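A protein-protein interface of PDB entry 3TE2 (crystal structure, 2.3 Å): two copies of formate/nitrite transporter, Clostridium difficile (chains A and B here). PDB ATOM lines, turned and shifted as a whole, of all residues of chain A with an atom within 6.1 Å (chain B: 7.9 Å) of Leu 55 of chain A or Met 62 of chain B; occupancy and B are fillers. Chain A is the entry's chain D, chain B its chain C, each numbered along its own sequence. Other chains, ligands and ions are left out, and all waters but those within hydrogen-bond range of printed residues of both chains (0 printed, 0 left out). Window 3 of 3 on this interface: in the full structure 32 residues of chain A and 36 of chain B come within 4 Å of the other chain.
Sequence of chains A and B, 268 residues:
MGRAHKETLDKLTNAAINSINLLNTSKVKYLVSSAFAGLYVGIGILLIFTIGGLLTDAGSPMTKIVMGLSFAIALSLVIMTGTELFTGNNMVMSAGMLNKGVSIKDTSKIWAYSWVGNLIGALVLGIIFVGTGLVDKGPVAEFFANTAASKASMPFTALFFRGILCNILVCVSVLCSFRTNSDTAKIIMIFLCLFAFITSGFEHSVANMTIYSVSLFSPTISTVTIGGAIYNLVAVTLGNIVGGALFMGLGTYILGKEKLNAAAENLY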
ATOM      1  N   THR A  50     -26.078   2.004  24.347  1.00  0.00           N
ATOM      2  CA  THR A  50     -25.042   2.228  23.349  1.00  0.00           C
ATOM      3  C   THR A  50     -24.831   0.931  22.579  1.00  0.00           C
ATOM      4  O   THR A  50     -24.803   0.923  21.348  1.00  0.00           O
ATOM      5  CB  THR A  50     -23.714   2.666  23.984  1.00  0.00           C
ATOM      6  OG1 THR A  50     -23.895   3.922  24.649  1.00  0.00           O
ATOM      7  CG2 THR A  50     -22.644   2.822  22.911  1.00  0.00           C
ATOM      8  N   ILE A  51     -24.694  -0.164  23.323  1.00  0.00           N
ATOM      9  CA  ILE A  51     -24.585  -1.499  22.751  1.00  0.00           C
ATOM     10  C   ILE A  51     -25.804  -1.810  21.884  1.00  0.00           C
ATOM     11  O   ILE A  51     -25.670  -2.191  20.720  1.00  0.00           O
ATOM     12  CB  ILE A  51     -24.421  -2.567  23.863  1.00  0.00           C
ATOM     13  CG1 ILE A  51     -23.025  -2.474  24.486  1.00  0.00           C
ATOM     14  CG2 ILE A  51     -24.666  -3.967  23.323  1.00  0.00           C
ATOM     15  CD1 ILE A  51     -22.832  -3.358  25.703  1.00  0.00           C
ATOM     16  N   GLY A  52     -26.995  -1.633  22.451  1.00  0.00           N
ATOM     17  CA  GLY A  52     -28.229  -1.848  21.711  1.00  0.00           C
ATOM     18  C   GLY A  52     -28.231  -1.130  20.374  1.00  0.00           C
ATOM     19  O   GLY A  52     -28.545  -1.719  19.336  1.00  0.00           O
ATOM     20  N   GLY A  53     -27.872   0.149  20.394  1.00  0.00           N
ATOM     21  CA  GLY A  53     -27.787   0.928  19.174  1.00  0.00           C
ATOM     22  C   GLY A  53     -26.816   0.327  18.174  1.00  0.00           C
ATOM     23  O   GLY A  53     -27.179   0.066  17.023  1.00  0.00           O
ATOM     24  N   LEU A  54     -25.580   0.102  18.615  1.00  0.00           N
ATOM     25  CA  LEU A  54     -24.541  -0.435  17.738  1.00  0.00           C
ATOM     26  C   LEU A  54     -24.956  -1.752  17.082  1.00  0.00           C
ATOM     27  O   LEU A  54     -24.840  -1.915  15.868  1.00  0.00           O
ATOM     28  CB  LEU A  54     -23.223  -0.609  18.504  1.00  0.00           C
ATOM     29  CG  LEU A  54     -22.450   0.672  18.844  1.00  0.00           C
ATOM     30  CD1 LEU A  54     -21.362   0.403  19.878  1.00  0.00           C
ATOM     31  CD2 LEU A  54     -21.860   1.303  17.583  1.00  0.00           C
ATOM     32  N   LEU A  55     -25.450  -2.686  17.889  1.00  0.00           N
ATOM     33  CA  LEU A  55     -25.799  -4.018  17.402  1.00  0.00           C
ATOM     34  C   LEU A  55     -27.154  -4.067  16.682  1.00  0.00           C
ATOM     35  O   LEU A  55     -27.367  -4.899  15.800  1.00  0.00           O
ATOM     36  CB  LEU A  55     -25.756  -5.028  18.553  1.00  0.00           C
ATOM     37  CG  LEU A  55     -24.390  -5.124  19.246  1.00  0.00           C
ATOM     38  CD1 LEU A  55     -24.389  -6.208  20.312  1.00  0.00           C
ATOM     39  CD2 LEU A  55     -23.295  -5.388  18.223  1.00  0.00           C
ATOM     40  N   THR A  56     -28.073  -3.186  17.066  1.00  0.00           N
ATOM     41  CA  THR A  56     -29.339  -3.076  16.349  1.00  0.00           C
ATOM     42  C   THR A  56     -29.074  -2.615  14.921  1.00  0.00           C
ATOM     43  O   THR A  56     -29.612  -3.175  13.965  1.00  0.00           O
ATOM     44  CB  THR A  56     -30.310  -2.093  17.036  1.00  0.00           C
ATOM     45  OG1 THR A  56     -30.831  -2.685  18.235  1.00  0.00           O
ATOM     46  CG2 THR A  56     -31.460  -1.754  16.111  1.00  0.00           C
ATOM     47  N   ASP A  57     -28.225  -1.600  14.790  1.00  0.00           N
ATOM     48  CA  ASP A  57     -27.879  -1.021  13.494  1.00  0.00           C
ATOM     49  C   ASP A  57     -27.131  -2.020  12.613  1.00  0.00           C
ATOM     50  O   ASP A  57     -27.028  -1.838  11.398  1.00  0.00           O
ATOM     51  CB  ASP A  57     -27.030   0.238  13.696  1.00  0.00           C
ATOM     52  CG  ASP A  57     -26.856   1.043  12.424  1.00  0.00           C
ATOM     53  OD1 ASP A  57     -27.841   1.198  11.668  1.00  0.00           O
ATOM     54  OD2 ASP A  57     -25.729   1.528  12.181  1.00  0.00           O
ATOM     55  N   ALA A  58     -26.614  -3.078  13.231  1.00  0.00           N
ATOM     56  CA  ALA A  58     -25.836  -4.088  12.521  1.00  0.00           C
ATOM     57  C   ALA A  58     -26.688  -5.289  12.131  1.00  0.00           C
ATOM     58  O   ALA A  58     -26.271  -6.122  11.326  1.00  0.00           O
ATOM     59  CB  ALA A  58     -24.654  -4.535  13.371  1.00  0.00           C
ATOM     60  N   GLY A  59     -27.881  -5.379  12.708  1.00  0.00           N
ATOM     61  CA  GLY A  59     -28.764  -6.502  12.453  1.00  0.00           C
ATOM     62  C   GLY A  59     -28.313  -7.768  13.157  1.00  0.00           C
ATOM     63  O   GLY A  59     -28.638  -8.878  12.732  1.00  0.00           O
ATOM     64  N   SER A  60     -27.560  -7.601  14.240  1.00  0.00           N
ATOM     65  CA  SER A  60     -27.068  -8.734  15.016  1.00  0.00           C
ATOM     66  C   SER A  60     -28.172  -9.368  15.853  1.00  0.00           C
ATOM     67  O   SER A  60     -28.898  -8.674  16.560  1.00  0.00           O
ATOM     68  CB  SER A  60     -25.922  -8.294  15.929  1.00  0.00           C
ATOM     69  OG  SER A  60     -25.736  -9.212  16.992  1.00  0.00           O
ATOM     70  N   PRO A  61     -28.296 -10.699  15.775  1.00  0.00           N
ATOM     71  CA  PRO A  61     -29.245 -11.451  16.605  1.00  0.00           C
ATOM     72  C   PRO A  61     -28.803 -11.552  18.068  1.00  0.00           C
ATOM     73  O   PRO A  61     -29.565 -12.051  18.897  1.00  0.00           O
ATOM     74  CB  PRO A  61     -29.245 -12.838  15.959  1.00  0.00           C
ATOM     75  CG  PRO A  61     -27.909 -12.943  15.302  1.00  0.00           C
ATOM     76  CD  PRO A  61     -27.584 -11.564  14.818  1.00  0.00           C
ATOM     77  N   MET A  62     -27.598 -11.080  18.379  1.00  0.00           N
ATOM     78  CA  MET A  62     -27.039 -11.205  19.728  1.00  0.00           C
ATOM     79  C   MET A  62     -27.282  -9.963  20.592  1.00  0.00           C
ATOM     80  O   MET A  62     -26.924  -9.938  21.769  1.00  0.00           O
ATOM     81  CB  MET A  62     -25.534 -11.511  19.656  1.00  0.00           C
ATOM     82  CG  MET A  62     -25.191 -12.909  19.125  1.00  0.00           C
ATOM     83  SD  MET A  62     -25.387 -14.225  20.357  1.00  0.00           S
ATOM     84  CE  MET A  62     -24.169 -13.737  21.575  1.00  0.00           C
ATOM     85  N   THR A  63     -27.893  -8.942  19.999  1.00  0.00           N
ATOM     86  CA  THR A  63     -28.128  -7.661  20.665  1.00  0.00           C
ATOM     87  C   THR A  63     -28.619  -7.790  22.111  1.00  0.00           C
ATOM     88  O   THR A  63     -27.962  -7.319  23.039  1.00  0.00           O
ATOM     89  CB  THR A  63     -29.132  -6.788  19.861  1.00  0.00           C
ATOM     90  OG1 THR A  63     -28.581  -6.491  18.577  1.00  0.00           O
ATOM     91  CG2 THR A  63     -29.420  -5.478  20.586  1.00  0.00           C
ATOM     92  N   VAL A  66     -26.169  -9.669  24.444  1.00  0.00           N
ATOM     93  CA  VAL A  66     -25.024  -8.843  24.826  1.00  0.00           C
ATOM     94  C   VAL A  66     -25.430  -7.724  25.789  1.00  0.00           C
ATOM     95  O   VAL A  66     -24.685  -7.380  26.707  1.00  0.00           O
ATOM     96  CB  VAL A  66     -24.322  -8.235  23.590  1.00  0.00           C
ATOM     97  CG1 VAL A  66     -23.123  -7.405  24.019  1.00  0.00           C
ATOM     98  CG2 VAL A  66     -23.889  -9.335  22.638  1.00  0.00           C
ATOM     99  N   MET A  67     -26.611  -7.155  25.571  1.00  0.00           N
ATOM    100  CA  MET A  67     -27.148  -6.146  26.473  1.00  0.00           C
ATOM    101  C   MET A  67     -27.301  -6.721  27.883  1.00  0.00           C
ATOM    102  O   MET A  67     -26.881  -6.107  28.863  1.00  0.00           O
ATOM    103  CB  MET A  67     -28.492  -5.607  25.956  1.00  0.00           C
ATOM    104  CG  MET A  67     -28.374  -4.686  24.746  1.00  0.00           C
ATOM    105  SD  MET A  67     -29.952  -4.040  24.138  1.00  0.00           S
ATOM    106  CE  MET A  67     -30.520  -3.066  25.540  1.00  0.00           C
ATOM    107  N   ILE B  51      -6.718  -2.934  18.926  1.00  0.00           N
ATOM    108  CA  ILE B  51      -7.985  -3.595  18.665  1.00  0.00           C
ATOM    109  C   ILE B  51      -8.850  -2.728  17.753  1.00  0.00           C
ATOM    110  O   ILE B  51      -9.480  -3.230  16.822  1.00  0.00           O
ATOM    111  CB  ILE B  51      -8.710  -3.943  19.981  1.00  0.00           C
ATOM    112  CG1 ILE B  51      -7.962  -5.074  20.697  1.00  0.00           C
ATOM    113  CG2 ILE B  51     -10.148  -4.349  19.715  1.00  0.00           C
ATOM    114  CD1 ILE B  51      -8.416  -5.319  22.120  1.00  0.00           C
ATOM    115  N   LEU B  55     -10.180  -4.195  14.138  1.00  0.00           N
ATOM    116  CA  LEU B  55     -11.603  -4.448  13.936  1.00  0.00           C
ATOM    117  C   LEU B  55     -12.287  -3.374  13.092  1.00  0.00           C
ATOM    118  O   LEU B  55     -13.277  -3.649  12.412  1.00  0.00           O
ATOM    119  CB  LEU B  55     -12.321  -4.635  15.274  1.00  0.00           C
ATOM    120  CG  LEU B  55     -11.899  -5.879  16.060  1.00  0.00           C
ATOM    121  CD1 LEU B  55     -12.754  -6.055  17.306  1.00  0.00           C
ATOM    122  CD2 LEU B  55     -11.964  -7.126  15.184  1.00  0.00           C
ATOM    123  N   THR B  56     -11.763  -2.154  13.138  1.00  0.00           N
ATOM    124  CA  THR B  56     -12.270  -1.087  12.284  1.00  0.00           C
ATOM    125  C   THR B  56     -11.993  -1.439  10.830  1.00  0.00           C
ATOM    126  O   THR B  56     -12.864  -1.319   9.970  1.00  0.00           O
ATOM    127  CB  THR B  56     -11.617   0.274  12.610  1.00  0.00           C
ATOM    128  OG1 THR B  56     -12.149   0.779  13.841  1.00  0.00           O
ATOM    129  CG2 THR B  56     -11.894   1.277  11.500  1.00  0.00           C
ATOM    130  N   GLY B  59     -14.306  -3.828   9.428  1.00  0.00           N
ATOM    131  CA  GLY B  59     -15.694  -3.399   9.403  1.00  0.00           C
ATOM    132  C   GLY B  59     -16.553  -4.046  10.477  1.00  0.00           C
ATOM    133  O   GLY B  59     -17.759  -4.229  10.294  1.00  0.00           O
ATOM    134  N   SER B  60     -15.937  -4.385  11.605  1.00  0.00           N
ATOM    135  CA  SER B  60     -16.652  -5.049  12.689  1.00  0.00           C
ATOM    136  C   SER B  60     -17.566  -4.092  13.453  1.00  0.00           C
ATOM    137  O   SER B  60     -17.186  -2.958  13.746  1.00  0.00           O
ATOM    138  CB  SER B  60     -15.666  -5.710  13.656  1.00  0.00           C
ATOM    139  OG  SER B  60     -16.353  -6.390  14.694  1.00  0.00           O
ATOM    140  N   PRO B  61     -18.782  -4.552  13.778  1.00  0.00           N
ATOM    141  CA  PRO B  61     -19.708  -3.764  14.600  1.00  0.00           C
ATOM    142  C   PRO B  61     -19.419  -3.929  16.096  1.00  0.00           C
ATOM    143  O   PRO B  61     -19.899  -3.131  16.902  1.00  0.00           O
ATOM    144  CB  PRO B  61     -21.069  -4.364  14.251  1.00  0.00           C
ATOM    145  CG  PRO B  61     -20.765  -5.793  13.937  1.00  0.00           C
ATOM    146  CD  PRO B  61     -19.386  -5.814  13.315  1.00  0.00           C
ATOM    147  N   MET B  62     -18.637  -4.947  16.449  1.00  0.00           N
ATOM    148  CA  MET B  62     -18.298  -5.223  17.843  1.00  0.00           C
ATOM    149  C   MET B  62     -17.105  -4.394  18.317  1.00  0.00           C
ATOM    150  O   MET B  62     -16.686  -4.495  19.471  1.00  0.00           O
ATOM    151  CB  MET B  62     -17.993  -6.713  18.030  1.00  0.00           C
ATOM    152  CG  MET B  62     -19.202  -7.626  17.893  1.00  0.00           C
ATOM    153  SD  MET B  62     -20.261  -7.610  19.355  1.00  0.00           S
ATOM    154  CE  MET B  62     -19.114  -8.160  20.616  1.00  0.00           C
ATOM    155  N   THR B  63     -16.571  -3.573  17.419  1.00  0.00           N
ATOM    156  CA  THR B  63     -15.341  -2.833  17.668  1.00  0.00           C
ATOM    157  C   THR B  63     -15.300  -2.113  19.017  1.00  0.00           C
ATOM    158  O   THR B  63     -14.411  -2.363  19.834  1.00  0.00           O
ATOM    159  CB  THR B  63     -15.054  -1.825  16.525  1.00  0.00           C
ATOM    160  OG1 THR B  63     -14.728  -2.542  15.327  1.00  0.00           O
ATOM    161  CG2 THR B  63     -13.894  -0.914  16.887  1.00  0.00           C
ATOM    162  N   LYS B  64     -16.254  -1.218  19.247  1.00  0.00           N
ATOM    163  CA  LYS B  64     -16.249  -0.399  20.456  1.00  0.00           C
ATOM    164  C   LYS B  64     -16.621  -1.197  21.705  1.00  0.00           C
ATOM    165  O   LYS B  64     -16.334  -0.781  22.828  1.00  0.00           O
ATOM    166  CB  LYS B  64     -17.177   0.804  20.288  1.00  0.00           C
ATOM    167  CG  LYS B  64     -16.707   1.805  19.241  1.00  0.00           C
ATOM    168  CD  LYS B  64     -17.810   2.789  18.883  1.00  0.00           C
ATOM    169  CE  LYS B  64     -17.329   3.833  17.882  1.00  0.00           C
ATOM    170  NZ  LYS B  64     -18.442   4.718  17.435  1.00  0.00           N
ATOM    171  N   ILE B  65     -17.264  -2.341  21.505  1.00  0.00           N
ATOM    172  CA  ILE B  65     -17.626  -3.215  22.614  1.00  0.00           C
ATOM    173  C   ILE B  65     -16.390  -3.977  23.077  1.00  0.00           C
ATOM    174  O   ILE B  65     -16.073  -4.008  24.267  1.00  0.00           O
ATOM    175  CB  ILE B  65     -18.735  -4.211  22.208  1.00  0.00           C
ATOM    176  CG1 ILE B  65     -19.985  -3.456  21.747  1.00  0.00           C
ATOM    177  CG2 ILE B  65     -19.066  -5.151  23.360  1.00  0.00           C
ATOM    178  CD1 ILE B  65     -21.069  -4.358  21.187  1.00  0.00           C
ATOM    179  N   VAL B  66     -15.685  -4.577  22.123  1.00  0.00           N
ATOM    180  CA  VAL B  66     -14.446  -5.285  22.415  1.00  0.00           C
ATOM    181  C   VAL B  66     -13.383  -4.348  22.997  1.00  0.00           C
ATOM    182  O   VAL B  66     -12.613  -4.744  23.867  1.00  0.00           O
ATOM    183  CB  VAL B  66     -13.911  -6.011  21.163  1.00  0.00           C
ATOM    184  CG1 VAL B  66     -12.640  -6.777  21.490  1.00  0.00           C
ATOM    185  CG2 VAL B  66     -14.974  -6.953  20.617  1.00  0.00           C
ATOM    186  N   MET B  67     -13.351  -3.102  22.533  1.00  0.00           N
ATOM    187  CA  MET B  67     -12.407  -2.128  23.068  1.00  0.00           C
ATOM    188  C   MET B  67     -12.701  -1.849  24.537  1.00  0.00           C
ATOM    189  O   MET B  67     -11.789  -1.811  25.369  1.00  0.00           O
ATOM    190  CB  MET B  67     -12.440  -0.819  22.268  1.00  0.00           C
ATOM    191  CG  MET B  67     -11.791  -0.898  20.884  1.00  0.00           C
ATOM    192  SD  MET B  67     -11.928   0.646  19.945  1.00  0.00           S
ATOM    193  CE  MET B  67     -10.942   1.759  20.944  1.00  0.00           C
ATOM    194  N   GLY B  68     -13.977  -1.644  24.852  1.00  0.00           N
ATOM    195  CA  GLY B  68     -14.384  -1.383  26.223  1.00  0.00           C
ATOM    196  C   GLY B  68     -14.062  -2.545  27.148  1.00  0.00           C
ATOM    197  O   GLY B  68     -13.559  -2.350  28.253  1.00  0.00           O
ATOM    198  N   LEU B  69     -14.344  -3.761  26.691  1.00  0.00           N
ATOM    199  CA  LEU B  69     -14.082  -4.957  27.484  1.00  0.00           C
ATOM    200  C   LEU B  69     -12.594  -5.132  27.757  1.00  0.00           C
ATOM    201  O   LEU B  69     -12.208  -5.760  28.743  1.00  0.00           O
ATOM    202  CB  LEU B  69     -14.623  -6.201  26.770  1.00  0.00           C
ATOM    203  CG  LEU B  69     -16.148  -6.320  26.651  1.00  0.00           C
ATOM    204  CD1 LEU B  69     -16.519  -7.437  25.696  1.00  0.00           C
ATOM    205  CD2 LEU B  69     -16.779  -6.550  28.024  1.00  0.00           C
ATOM    206  N   THR B 199     -16.839   2.160  26.152  1.00  0.00           N
ATOM    207  CA  THR B 199     -17.854   1.859  25.144  1.00  0.00           C
ATOM    208  C   THR B 199     -18.892   2.982  24.987  1.00  0.00           C
ATOM    209  O   THR B 199     -19.303   3.303  23.870  1.00  0.00           O
ATOM    210  CB  THR B 199     -18.558   0.516  25.431  1.00  0.00           C
ATOM    211  OG1 THR B 199     -17.603  -0.549  25.362  1.00  0.00           O
ATOM    212  CG2 THR B 199     -19.666   0.264  24.417  1.00  0.00           C
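Leu 55 of chain A touches Met 62 of chain B, but with the chains exchanged Met 62 of chain A does not touch Leu 55 of chain B (14.1 Å).
Of chain B, only Met 62 and Ile 65 come within 4 Å of Leu 55 of chain A. Of chain A, only Leu 55 comes within 4 Å of Met 62 of chain B. Of the printed residues of chain B, Ala 58 of chain A touches Pro 61 (3.7 Å). Of the printed residues of chain B, Thr 50 of chain A touches Thr 199. Printed residues of chain A within 4 Å of Ile 65 of chain B: Leu 55. Printed residues of chain A within 4 Å of Thr 199 of chain B: Thr 50 (3.5 Å). Printed residues of chain A within 4 Å of Pro 61 of chain B: Ala 58. The nearest residue of chain B that does not touch Leu 55 of chain A is Pro 61 of chain B (4.3 Å). The nearest printed residue of chain A that does not touch Ile 65 of chain B is Ile 51 of chain A (4.2 Å).
Among the printed residues, pairs that only touch across the chains: Thr 50 of chain A with Thr 199 of chain B (3.5 Å), Leu 55 of chain A with Met 62 of chain B (3.9 Å), Leu 55 of chain A with Ile 65 of chain B (3.8 Å) and Ala 58 of chain A with Pro 61 of chain B (3.7 Å).
OG1 of Thr 63 of chain A sits close to O of Leu 55 of chain A, 3.4 Å away. The side-chain hydroxyl (OG1) of Thr 199 of chain B lies within hydrogen-bond range of the backbone carbonyl oxygen (O) of Lys 64 of chain B (2.8 Å). The side-chain hydroxyl (OG) of Ser 60 of chain B is in hydrogen-bond range of the backbone NH (N) of Met 62 of chain B. The backbone carbonyl oxygen (O) of Leu 55 of chain A sits at hydrogen-bond distance from the backbone NH (N) of Ser 60 of chain A, 3.1 Å away.
Printed residues of chain A that touch a printed residue of chain B: Thr 50, Leu 55 and Ala 58. Among the printed residues, no Asp or Glu carboxylate lies within 4 Å of a Lys or Arg side-chain nitrogen of the other chain.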
